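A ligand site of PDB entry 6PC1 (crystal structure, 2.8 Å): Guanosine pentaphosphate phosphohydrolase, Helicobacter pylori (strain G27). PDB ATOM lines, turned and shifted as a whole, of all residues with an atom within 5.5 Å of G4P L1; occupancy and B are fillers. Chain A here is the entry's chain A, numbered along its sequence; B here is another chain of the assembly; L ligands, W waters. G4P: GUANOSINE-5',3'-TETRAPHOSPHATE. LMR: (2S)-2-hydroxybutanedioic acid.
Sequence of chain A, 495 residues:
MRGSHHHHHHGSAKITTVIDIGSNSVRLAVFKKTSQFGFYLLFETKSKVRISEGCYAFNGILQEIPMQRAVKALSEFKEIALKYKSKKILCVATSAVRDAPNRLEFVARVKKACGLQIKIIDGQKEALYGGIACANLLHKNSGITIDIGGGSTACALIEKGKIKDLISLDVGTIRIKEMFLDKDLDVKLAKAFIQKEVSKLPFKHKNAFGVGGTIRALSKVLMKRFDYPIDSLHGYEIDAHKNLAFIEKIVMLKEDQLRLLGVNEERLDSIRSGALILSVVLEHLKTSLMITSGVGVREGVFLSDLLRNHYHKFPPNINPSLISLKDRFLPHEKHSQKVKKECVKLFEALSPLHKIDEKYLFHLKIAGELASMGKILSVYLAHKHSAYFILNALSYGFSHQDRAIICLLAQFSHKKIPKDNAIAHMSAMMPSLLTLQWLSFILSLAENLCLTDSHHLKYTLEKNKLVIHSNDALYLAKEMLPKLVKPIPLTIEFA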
ATOM      1  N   ARG A  27      -4.588  -5.291   0.003  1.00  0.00           N
ATOM      2  CA  ARG A  27      -4.803  -4.515  -1.215  1.00  0.00           C
ATOM      3  C   ARG A  27      -4.899  -3.025  -0.902  1.00  0.00           C
ATOM      4  O   ARG A  27      -5.420  -2.615   0.139  1.00  0.00           O
ATOM      5  CB  ARG A  27      -6.087  -4.976  -1.923  1.00  0.00           C
ATOM      6  CG  ARG A  27      -6.084  -6.447  -2.311  1.00  0.00           C
ATOM      7  CD  ARG A  27      -5.454  -6.656  -3.671  1.00  0.00           C
ATOM      8  NE  ARG A  27      -5.361  -8.067  -4.033  1.00  0.00           N
ATOM      9  CZ  ARG A  27      -4.936  -8.516  -5.206  1.00  0.00           C
ATOM     10  NH1 ARG A  27      -4.564  -7.658  -6.153  1.00  0.00           N
ATOM     11  NH2 ARG A  27      -4.881  -9.819  -5.447  1.00  0.00           N
ATOM     12  N   GLU A  44      -3.036   1.346  -7.863  1.00  0.00           N
ATOM     13  CA  GLU A  44      -3.386   0.112  -7.181  1.00  0.00           C
ATOM     14  C   GLU A  44      -2.120  -0.694  -6.943  1.00  0.00           C
ATOM     15  O   GLU A  44      -1.196  -0.669  -7.754  1.00  0.00           O
ATOM     16  CB  GLU A  44      -4.399  -0.706  -8.002  1.00  0.00           C
ATOM     17  CG  GLU A  44      -5.171  -1.743  -7.205  1.00  0.00           C
ATOM     18  CD  GLU A  44      -6.208  -2.449  -8.056  1.00  0.00           C
ATOM     19  OE1 GLU A  44      -6.031  -2.472  -9.288  1.00  0.00           O
ATOM     20  OE2 GLU A  44      -7.200  -2.955  -7.495  1.00  0.00           O
ATOM     21  N   LYS A  46      -0.606  -4.319  -4.234  1.00  0.00           N
ATOM     22  CA  LYS A  46      -0.973  -5.428  -3.365  1.00  0.00           C
ATOM     23  C   LYS A  46       0.254  -5.926  -2.625  1.00  0.00           C
ATOM     24  O   LYS A  46       1.392  -5.604  -2.958  1.00  0.00           O
ATOM     25  CB  LYS A  46      -1.617  -6.573  -4.163  1.00  0.00           C
ATOM     26  CG  LYS A  46      -0.617  -7.480  -4.886  1.00  0.00           C
ATOM     27  CD  LYS A  46      -1.107  -7.910  -6.262  1.00  0.00           C
ATOM     28  CE  LYS A  46      -1.041  -6.770  -7.263  1.00  0.00           C
ATOM     29  NZ  LYS A  46      -1.339  -7.210  -8.657  1.00  0.00           N
ATOM     30  N   GLY A 213      -9.957 -12.335  -6.824  1.00  0.00           N
ATOM     31  CA  GLY A 213      -8.802 -12.674  -7.625  1.00  0.00           C
ATOM     32  C   GLY A 213      -8.810 -14.108  -8.131  1.00  0.00           C
ATOM     33  O   GLY A 213      -8.254 -14.393  -9.190  1.00  0.00           O
ATOM     34  N   ARG A 216     -10.962 -13.933 -11.208  1.00  0.00           N
ATOM     35  CA  ARG A 216     -10.205 -13.203 -12.215  1.00  0.00           C
ATOM     36  C   ARG A 216      -9.106 -14.078 -12.801  1.00  0.00           C
ATOM     37  O   ARG A 216      -8.825 -14.026 -14.007  1.00  0.00           O
ATOM     38  CB  ARG A 216      -9.605 -11.930 -11.623  1.00  0.00           C
ATOM     39  CG  ARG A 216     -10.632 -10.868 -11.227  1.00  0.00           C
ATOM     40  CD  ARG A 216      -9.987  -9.506 -11.025  1.00  0.00           C
ATOM     41  NE  ARG A 216      -8.745  -9.597 -10.264  1.00  0.00           N
ATOM     42  CZ  ARG A 216      -8.628  -9.425  -8.949  1.00  0.00           C
ATOM     43  NH1 ARG A 216      -9.694  -9.143  -8.207  1.00  0.00           N
ATOM     44  NH2 ARG A 216      -7.441  -9.542  -8.371  1.00  0.00           N
ATOM     45  N   LYS A 220      -9.107 -15.256 -16.644  1.00  0.00           N
ATOM     46  CA  LYS A 220      -7.899 -15.068 -17.451  1.00  0.00           C
ATOM     47  C   LYS A 220      -7.505 -16.361 -18.145  1.00  0.00           C
ATOM     48  O   LYS A 220      -7.009 -16.344 -19.276  1.00  0.00           O
ATOM     49  CB  LYS A 220      -6.774 -14.563 -16.559  1.00  0.00           C
ATOM     50  CG  LYS A 220      -5.701 -13.767 -17.278  1.00  0.00           C
ATOM     51  CD  LYS A 220      -4.517 -13.469 -16.358  1.00  0.00           C
ATOM     52  CE  LYS A 220      -4.934 -12.707 -15.098  1.00  0.00           C
ATOM     53  NZ  LYS A 220      -3.756 -12.361 -14.249  1.00  0.00           N
ATOM     54  N   LEU A 233     -10.615  -7.744 -18.458  1.00  0.00           N
ATOM     55  CA  LEU A 233     -11.325  -8.712 -17.629  1.00  0.00           C
ATOM     56  C   LEU A 233     -12.753  -8.258 -17.318  1.00  0.00           C
ATOM     57  O   LEU A 233     -13.692  -9.061 -17.386  1.00  0.00           O
ATOM     58  CB  LEU A 233     -10.569  -8.962 -16.316  1.00  0.00           C
ATOM     59  CG  LEU A 233      -9.288  -9.779 -16.386  1.00  0.00           C
ATOM     60  CD1 LEU A 233      -8.607  -9.801 -15.033  1.00  0.00           C
ATOM     61  CD2 LEU A 233      -9.585 -11.202 -16.851  1.00  0.00           C
ATOM     62  N   HIS A 234     -12.916  -6.990 -16.948  1.00  0.00           N
ATOM     63  CA  HIS A 234     -14.227  -6.496 -16.545  1.00  0.00           C
ATOM     64  C   HIS A 234     -15.226  -6.641 -17.675  1.00  0.00           C
ATOM     65  O   HIS A 234     -14.984  -6.194 -18.805  1.00  0.00           O
ATOM     66  CB  HIS A 234     -14.112  -5.035 -16.112  1.00  0.00           C
ATOM     67  CG  HIS A 234     -15.374  -4.489 -15.508  1.00  0.00           C
ATOM     68  ND1 HIS A 234     -15.815  -4.849 -14.255  1.00  0.00           N
ATOM     69  CD2 HIS A 234     -16.296  -3.628 -15.990  1.00  0.00           C
ATOM     70  CE1 HIS A 234     -16.940  -4.221 -13.985  1.00  0.00           C
ATOM     71  NE2 HIS A 234     -17.257  -3.468 -15.026  1.00  0.00           N
ATOM     72  N   ASN A 264      -0.348 -17.469 -12.615  1.00  0.00           N
ATOM     73  CA  ASN A 264       0.920 -17.007 -12.070  1.00  0.00           C
ATOM     74  C   ASN A 264       1.297 -17.823 -10.829  1.00  0.00           C
ATOM     75  O   ASN A 264       0.475 -18.549 -10.248  1.00  0.00           O
ATOM     76  CB  ASN A 264       0.867 -15.513 -11.750  1.00  0.00           C
ATOM     77  CG  ASN A 264      -0.192 -15.165 -10.721  1.00  0.00           C
ATOM     78  OD1 ASN A 264      -0.601 -16.013  -9.917  1.00  0.00           O
ATOM     79  ND2 ASN A 264      -0.628 -13.912 -10.723  1.00  0.00           N
ATOM     80  N   GLU A 266       1.987 -17.143  -7.714  1.00  0.00           N
ATOM     81  CA  GLU A 266       1.358 -16.874  -6.428  1.00  0.00           C
ATOM     82  C   GLU A 266      -0.095 -17.347  -6.358  1.00  0.00           C
ATOM     83  O   GLU A 266      -0.660 -17.370  -5.260  1.00  0.00           O
ATOM     84  CB  GLU A 266       1.439 -15.373  -6.116  1.00  0.00           C
ATOM     85  CG  GLU A 266       0.973 -14.437  -7.233  1.00  0.00           C
ATOM     86  CD  GLU A 266       1.528 -13.026  -7.084  1.00  0.00           C
ATOM     87  OE1 GLU A 266       2.332 -12.801  -6.148  1.00  0.00           O
ATOM     88  OE2 GLU A 266       1.151 -12.153  -7.895  1.00  0.00           O
ATOM     89  N   ARG A 267      -0.699 -17.721  -7.482  1.00  0.00           N
ATOM     90  CA  ARG A 267      -2.045 -18.278  -7.495  1.00  0.00           C
ATOM     91  C   ARG A 267      -2.060 -19.806  -7.613  1.00  0.00           C
ATOM     92  O   ARG A 267      -3.136 -20.405  -7.531  1.00  0.00           O
ATOM     93  CB  ARG A 267      -2.864 -17.697  -8.655  1.00  0.00           C
ATOM     94  CG  ARG A 267      -3.284 -16.246  -8.471  1.00  0.00           C
ATOM     95  CD  ARG A 267      -4.473 -16.122  -7.533  1.00  0.00           C
ATOM     96  NE  ARG A 267      -4.789 -14.728  -7.245  1.00  0.00           N
ATOM     97  CZ  ARG A 267      -5.643 -14.333  -6.300  1.00  0.00           C
ATOM     98  NH1 ARG A 267      -6.267 -15.230  -5.545  1.00  0.00           N
ATOM     99  NH2 ARG A 267      -5.861 -13.042  -6.115  1.00  0.00           N
ATOM    100  N   SER A 293     -16.211  -9.776 -12.980  1.00  0.00           N
ATOM    101  CA  SER A 293     -16.217  -8.425 -12.444  1.00  0.00           C
ATOM    102  C   SER A 293     -14.813  -8.056 -11.988  1.00  0.00           C
ATOM    103  O   SER A 293     -14.202  -8.774 -11.182  1.00  0.00           O
ATOM    104  CB  SER A 293     -17.195  -8.288 -11.282  1.00  0.00           C
ATOM    105  OG  SER A 293     -17.264  -6.952 -10.824  1.00  0.00           O
ATOM    106  N   GLY A 294     -14.301  -6.941 -12.498  1.00  0.00           N
ATOM    107  CA  GLY A 294     -13.038  -6.396 -12.045  1.00  0.00           C
ATOM    108  C   GLY A 294     -13.137  -5.518 -10.823  1.00  0.00           C
ATOM    109  O   GLY A 294     -12.109  -5.055 -10.321  1.00  0.00           O
ATOM    110  N   VAL A 295     -14.345  -5.266 -10.320  1.00  0.00           N
ATOM    111  CA  VAL A 295     -14.570  -4.457  -9.140  1.00  0.00           C
ATOM    112  C   VAL A 295     -15.104  -5.351  -8.027  1.00  0.00           C
ATOM    113  O   VAL A 295     -15.749  -6.373  -8.292  1.00  0.00           O
ATOM    114  CB  VAL A 295     -15.544  -3.290  -9.422  1.00  0.00           C
ATOM    115  CG1 VAL A 295     -15.008  -2.417 -10.546  1.00  0.00           C
ATOM    116  CG2 VAL A 295     -16.936  -3.828  -9.782  1.00  0.00           C
ATOM    117  N   ARG A 298     -13.390  -3.303  -2.494  1.00  0.00           N
ATOM    118  CA  ARG A 298     -12.708  -2.016  -2.472  1.00  0.00           C
ATOM    119  C   ARG A 298     -13.539  -0.933  -3.156  1.00  0.00           C
ATOM    120  O   ARG A 298     -13.704   0.167  -2.633  1.00  0.00           O
ATOM    121  CB  ARG A 298     -11.330  -2.140  -3.126  1.00  0.00           C
ATOM    122  CG  ARG A 298     -10.311  -2.862  -2.262  1.00  0.00           C
ATOM    123  CD  ARG A 298      -8.986  -3.052  -2.982  1.00  0.00           C
ATOM    124  NE  ARG A 298      -9.095  -3.972  -4.112  1.00  0.00           N
ATOM    125  CZ  ARG A 298      -9.240  -5.289  -3.990  1.00  0.00           C
ATOM    126  NH1 ARG A 298      -9.296  -5.850  -2.791  1.00  0.00           N
ATOM    127  NH2 ARG A 298      -9.327  -6.042  -5.079  1.00  0.00           N
ATOM    128  N   TYR B 380      -4.598  -0.673 -15.614  1.00  0.00           N
ATOM    129  CA  TYR B 380      -4.341  -1.981 -16.192  1.00  0.00           C
ATOM    130  C   TYR B 380      -3.778  -1.817 -17.596  1.00  0.00           C
ATOM    131  O   TYR B 380      -4.319  -1.055 -18.404  1.00  0.00           O
ATOM    132  CB  TYR B 380      -5.630  -2.800 -16.198  1.00  0.00           C
ATOM    133  CG  TYR B 380      -6.311  -2.808 -14.850  1.00  0.00           C
ATOM    134  CD1 TYR B 380      -5.716  -3.431 -13.761  1.00  0.00           C
ATOM    135  CD2 TYR B 380      -7.529  -2.162 -14.655  1.00  0.00           C
ATOM    136  CE1 TYR B 380      -6.329  -3.428 -12.524  1.00  0.00           C
ATOM    137  CE2 TYR B 380      -8.133  -2.155 -13.417  1.00  0.00           C
ATOM    138  CZ  TYR B 380      -7.536  -2.788 -12.359  1.00  0.00           C
ATOM    139  OH  TYR B 380      -8.141  -2.780 -11.121  1.00  0.00           O
ATOM    140  N   LEU B 381      -2.681  -2.522 -17.873  1.00  0.00           N
ATOM    141  CA  LEU B 381      -1.902  -2.312 -19.095  1.00  0.00           C
ATOM    142  C   LEU B 381      -1.412  -0.874 -19.192  1.00  0.00           C
ATOM    143  O   LEU B 381      -1.278  -0.335 -20.296  1.00  0.00           O
ATOM    144  CB  LEU B 381      -2.724  -2.695 -20.333  1.00  0.00           C
ATOM    145  CG  LEU B 381      -3.229  -4.130 -20.363  1.00  0.00           C
ATOM    146  CD1 LEU B 381      -4.111  -4.356 -21.574  1.00  0.00           C
ATOM    147  CD2 LEU B 381      -2.067  -5.117 -20.356  1.00  0.00           C
ATOM    148  N   HIS B 383       1.522   0.469 -18.719  1.00  0.00           N
ATOM    149  CA  HIS B 383       2.757   0.624 -19.478  1.00  0.00           C
ATOM    150  C   HIS B 383       2.504   0.471 -20.969  1.00  0.00           C
ATOM    151  O   HIS B 383       3.100   1.192 -21.775  1.00  0.00           O
ATOM    152  CB  HIS B 383       3.790  -0.397 -18.993  1.00  0.00           C
ATOM    153  CG  HIS B 383       4.250  -0.156 -17.584  1.00  0.00           C
ATOM    154  ND1 HIS B 383       3.516  -0.556 -16.492  1.00  0.00           N
ATOM    155  CD2 HIS B 383       5.343   0.465 -17.102  1.00  0.00           C
ATOM    156  CE1 HIS B 383       4.157  -0.200 -15.389  1.00  0.00           C
ATOM    157  NE2 HIS B 383       5.268   0.416 -15.733  1.00  0.00           N
ATOM    158  N   LYS B 415       9.045  -7.125 -17.716  1.00  0.00           N
ATOM    159  CA  LYS B 415       8.781  -8.214 -18.636  1.00  0.00           C
ATOM    160  C   LYS B 415      10.023  -8.478 -19.473  1.00  0.00           C
ATOM    161  O   LYS B 415      10.967  -7.683 -19.501  1.00  0.00           O
ATOM    162  CB  LYS B 415       7.586  -7.908 -19.539  1.00  0.00           C
ATOM    163  CG  LYS B 415       6.292  -7.658 -18.786  1.00  0.00           C
ATOM    164  CD  LYS B 415       5.135  -7.381 -19.742  1.00  0.00           C
ATOM    165  CE  LYS B 415       3.879  -6.975 -18.984  1.00  0.00           C
ATOM    166  NZ  LYS B 415       2.722  -6.769 -19.897  1.00  0.00           N
HETATM  167  PB  G4P L   1       0.419  -6.208 -16.440  1.00  0.00           P
HETATM  168  O1B G4P L   1       0.430  -7.585 -16.996  1.00  0.00           O
HETATM  169  O2B G4P L   1       1.345  -5.280 -17.370  1.00  0.00           O
HETATM  170  O3B G4P L   1       1.021  -6.211 -14.947  1.00  0.00           O
HETATM  171  O3A G4P L   1      -1.071  -5.588 -16.430  1.00  0.00           O
HETATM  172  PA  G4P L   1      -2.167  -6.741 -16.153  1.00  0.00           P
HETATM  173  O1A G4P L   1      -3.521  -6.130 -16.206  1.00  0.00           O
HETATM  174  O2A G4P L   1      -2.074  -7.894 -17.276  1.00  0.00           O
HETATM  175  O5' G4P L   1      -1.946  -7.397 -14.694  1.00  0.00           O
HETATM  176  C5' G4P L   1      -2.052  -6.350 -13.721  1.00  0.00           C
HETATM  177  C4' G4P L   1      -2.865  -6.832 -12.520  1.00  0.00           C
HETATM  178  O4' G4P L   1      -4.196  -6.249 -12.569  1.00  0.00           O
HETATM  179  C3' G4P L   1      -3.090  -8.367 -12.517  1.00  0.00           C
HETATM  180  O3' G4P L   1      -3.264  -8.810 -11.170  1.00  0.00           O
HETATM  181  C2' G4P L   1      -4.426  -8.488 -13.265  1.00  0.00           C
HETATM  182  O2' G4P L   1      -5.038  -9.754 -13.016  1.00  0.00           O
HETATM  183  C1' G4P L   1      -5.154  -7.329 -12.570  1.00  0.00           C
HETATM  184  N9  G4P L   1      -6.381  -6.888 -13.250  1.00  0.00           N
HETATM  185  C8  G4P L   1      -6.614  -6.788 -14.586  1.00  0.00           C
HETATM  186  N7  G4P L   1      -7.811  -6.331 -14.783  1.00  0.00           N
HETATM  187  C5  G4P L   1      -8.414  -6.114 -13.592  1.00  0.00           C
HETATM  188  C6  G4P L   1      -9.690  -5.641 -13.196  1.00  0.00           C
HETATM  189  O6  G4P L   1     -10.529  -5.314 -14.021  1.00  0.00           O
HETATM  190  N1  G4P L   1      -9.948  -5.546 -11.873  1.00  0.00           N
HETATM  191  C2  G4P L   1      -9.017  -5.903 -10.953  1.00  0.00           C
HETATM  192  N2  G4P L   1      -9.305  -5.802  -9.611  1.00  0.00           N
HETATM  193  N3  G4P L   1      -7.831  -6.349 -11.313  1.00  0.00           N
HETATM  194  C4  G4P L   1      -7.503  -6.470 -12.595  1.00  0.00           C
HETATM  195  PC  G4P L   1      -2.161  -9.927 -10.821  1.00  0.00           P
HETATM  196  O1C G4P L   1      -0.806  -9.336 -10.952  1.00  0.00           O
HETATM  197  O2C G4P L   1      -2.293 -11.166 -11.835  1.00  0.00           O
HETATM  198  O3C G4P L   1      -2.382 -10.427  -9.311  1.00  0.00           O
HETATM  199  PD  G4P L   1      -3.946 -10.368  -8.925  1.00  0.00           P
HETATM  200  O1D G4P L   1      -4.790 -10.560 -10.123  1.00  0.00           O
HETATM  201  O2D G4P L   1      -4.255 -11.533  -7.863  1.00  0.00           O
HETATM  202  O3D G4P L   1      -4.295  -8.945  -8.247  1.00  0.00           O
HETATM  203  C1  LMR L   2      -9.229  -9.493  -4.038  1.00  0.00           C
HETATM  204  O1A LMR L   2      -8.914  -9.413  -5.204  1.00  0.00           O
HETATM  205  O1B LMR L   2      -9.847  -8.465  -3.436  1.00  0.00           O
HETATM  206  C2  LMR L   2      -8.923 -10.745  -3.257  1.00  0.00           C
HETATM  207  O2  LMR L   2      -9.990 -11.681  -3.418  1.00  0.00           O
HETATM  208  C3  LMR L   2      -7.622 -11.360  -3.747  1.00  0.00           C
HETATM  209  C4  LMR L   2      -7.503 -12.750  -3.178  1.00  0.00           C
HETATM  210  O4A LMR L   2      -8.439 -13.512  -3.244  1.00  0.00           O
HETATM  211  O4B LMR L   2      -6.360 -13.146  -2.610  1.00  0.00           O
HETATM  212  O   HOH W   1      -2.681 -13.218  -9.132  1.00  0.00           O
HETATM  213  O   HOH W   2      -7.585  -6.663 -17.774  1.00  0.00           O
HETATM  214  O   HOH W   3      -3.783 -13.791 -11.865  1.00  0.00           O
HETATM  215  O   HOH W   4      -5.892 -13.307 -10.190  1.00  0.00           O
HETATM  216  O   HOH W   5     -10.535  -5.187 -16.745  1.00  0.00           O
HETATM  217  O   HOH W   6      -0.619  -2.415 -15.608  1.00  0.00           O
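Water W1 lies within hydrogen-bond range of an oxygen (O2D) of G4P L1 (2.6 Å), the side-chain amide nitrogen (ND2) of Asn 264 (2.7 Å) and the guanidinium group (NE) of Arg 267 (3.2 Å).
Water W5 lies within hydrogen-bond range of an oxygen (O6) of G4P L1 (2.7 Å), the backbone NH of His 234 (3.0 Å) and the backbone NH of Leu 233 (3.1 Å).
Water W4 lies within hydrogen-bond range of the backbone carbonyl oxygen (O) of Gly 213, an oxygen (O1D) of G4P L1 and the guanidinium group (NE) of Arg 267.
Water W2 lies within hydrogen-bond range of N7 of G4P L1 and N of Leu 233.
Water W3 lies within hydrogen-bond range of the side-chain amino group (NZ) of Lys 220 (2.8 Å), an oxygen (O2C) of G4P L1 (3.0 Å) and the side-chain amide nitrogen (ND2) of Asn 264 (3.4 Å).
Water W6 lies within hydrogen-bond range of N of Leu 381 of chain B (3.1 Å) and O3A of G4P L1 (3.3 Å).
The side-chain amino group of Lys 415 of chain B lies within salt-bridge range of an oxygen (O2B) of G4P L1 (3.2 Å).
O of Gly 294 lies within hydrogen-bond range of N1 of G4P L1 (2.7 Å).
The backbone NH (N) of Gly 213 is in hydrogen-bond range of an oxygen (O2) of LMR L2 (3.5 Å).
NZ of Lys 46 is in salt-bridge range of O1C of G4P L1 (3.2 Å).
The guanidinium group (NH2) of Arg 267 is in salt-bridge range of an oxygen (O4B) of LMR L2, at 3.5 Å.
The side-chain amino group (NZ) of Lys 220 is in salt-bridge range of an oxygen (O2C) of G4P L1, at 3.1 Å.
The guanidinium group (NE) of Arg 27 lies within salt-bridge range of an oxygen (O1A) of LMR L2.
A nitrogen (N1) of G4P L1 lies close to the side-chain hydroxyl of Tyr 380 of chain B (3.4 Å).
NH1 of Arg 216 lies within salt-bridge range of O1A of LMR L2 (3.1 Å).
NH2 of Arg 267 lies within salt-bridge range of O2D of G4P L1, 2.8 Å away.
O3D of G4P L1 lies within salt-bridge range of NH1 of Arg 27.
NH1 of Arg 298 is in salt-bridge range of O1B of LMR L2, 2.7 Å away.
O3D of G4P L1 is in salt-bridge range of NH2 of Arg 216.
The side-chain amide nitrogen of Asn 264 is in hydrogen-bond range of an oxygen (O2C) of G4P L1.
Leu 233 touches G4P L1 (CD1 to N7, 3.6 Å).
Leu 381 of chain B touches G4P L1.
Hydrophobic or aromatic side chains that line G4P L1: Leu 233 and Tyr 380 of chain B.
Along chain A the residues within 4 Å of G4P L1 span positions 27 to 294.
The nearest printed residue that does not touch G4P L1 is Glu 44 (4.1 Å).
The side-chain hydroxyl of Tyr 380 of chain B is in hydrogen-bond range of the side-chain carboxylate of Glu 44 (2.8 Å).
The backbone NH (N) of Gly 294 is in hydrogen-bond range of a ring nitrogen (ND1) of His 234, 3.1 Å away.
N of Arg 267 lies within hydrogen-bond range of OD1 of Asn 264, 3.0 Å away.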
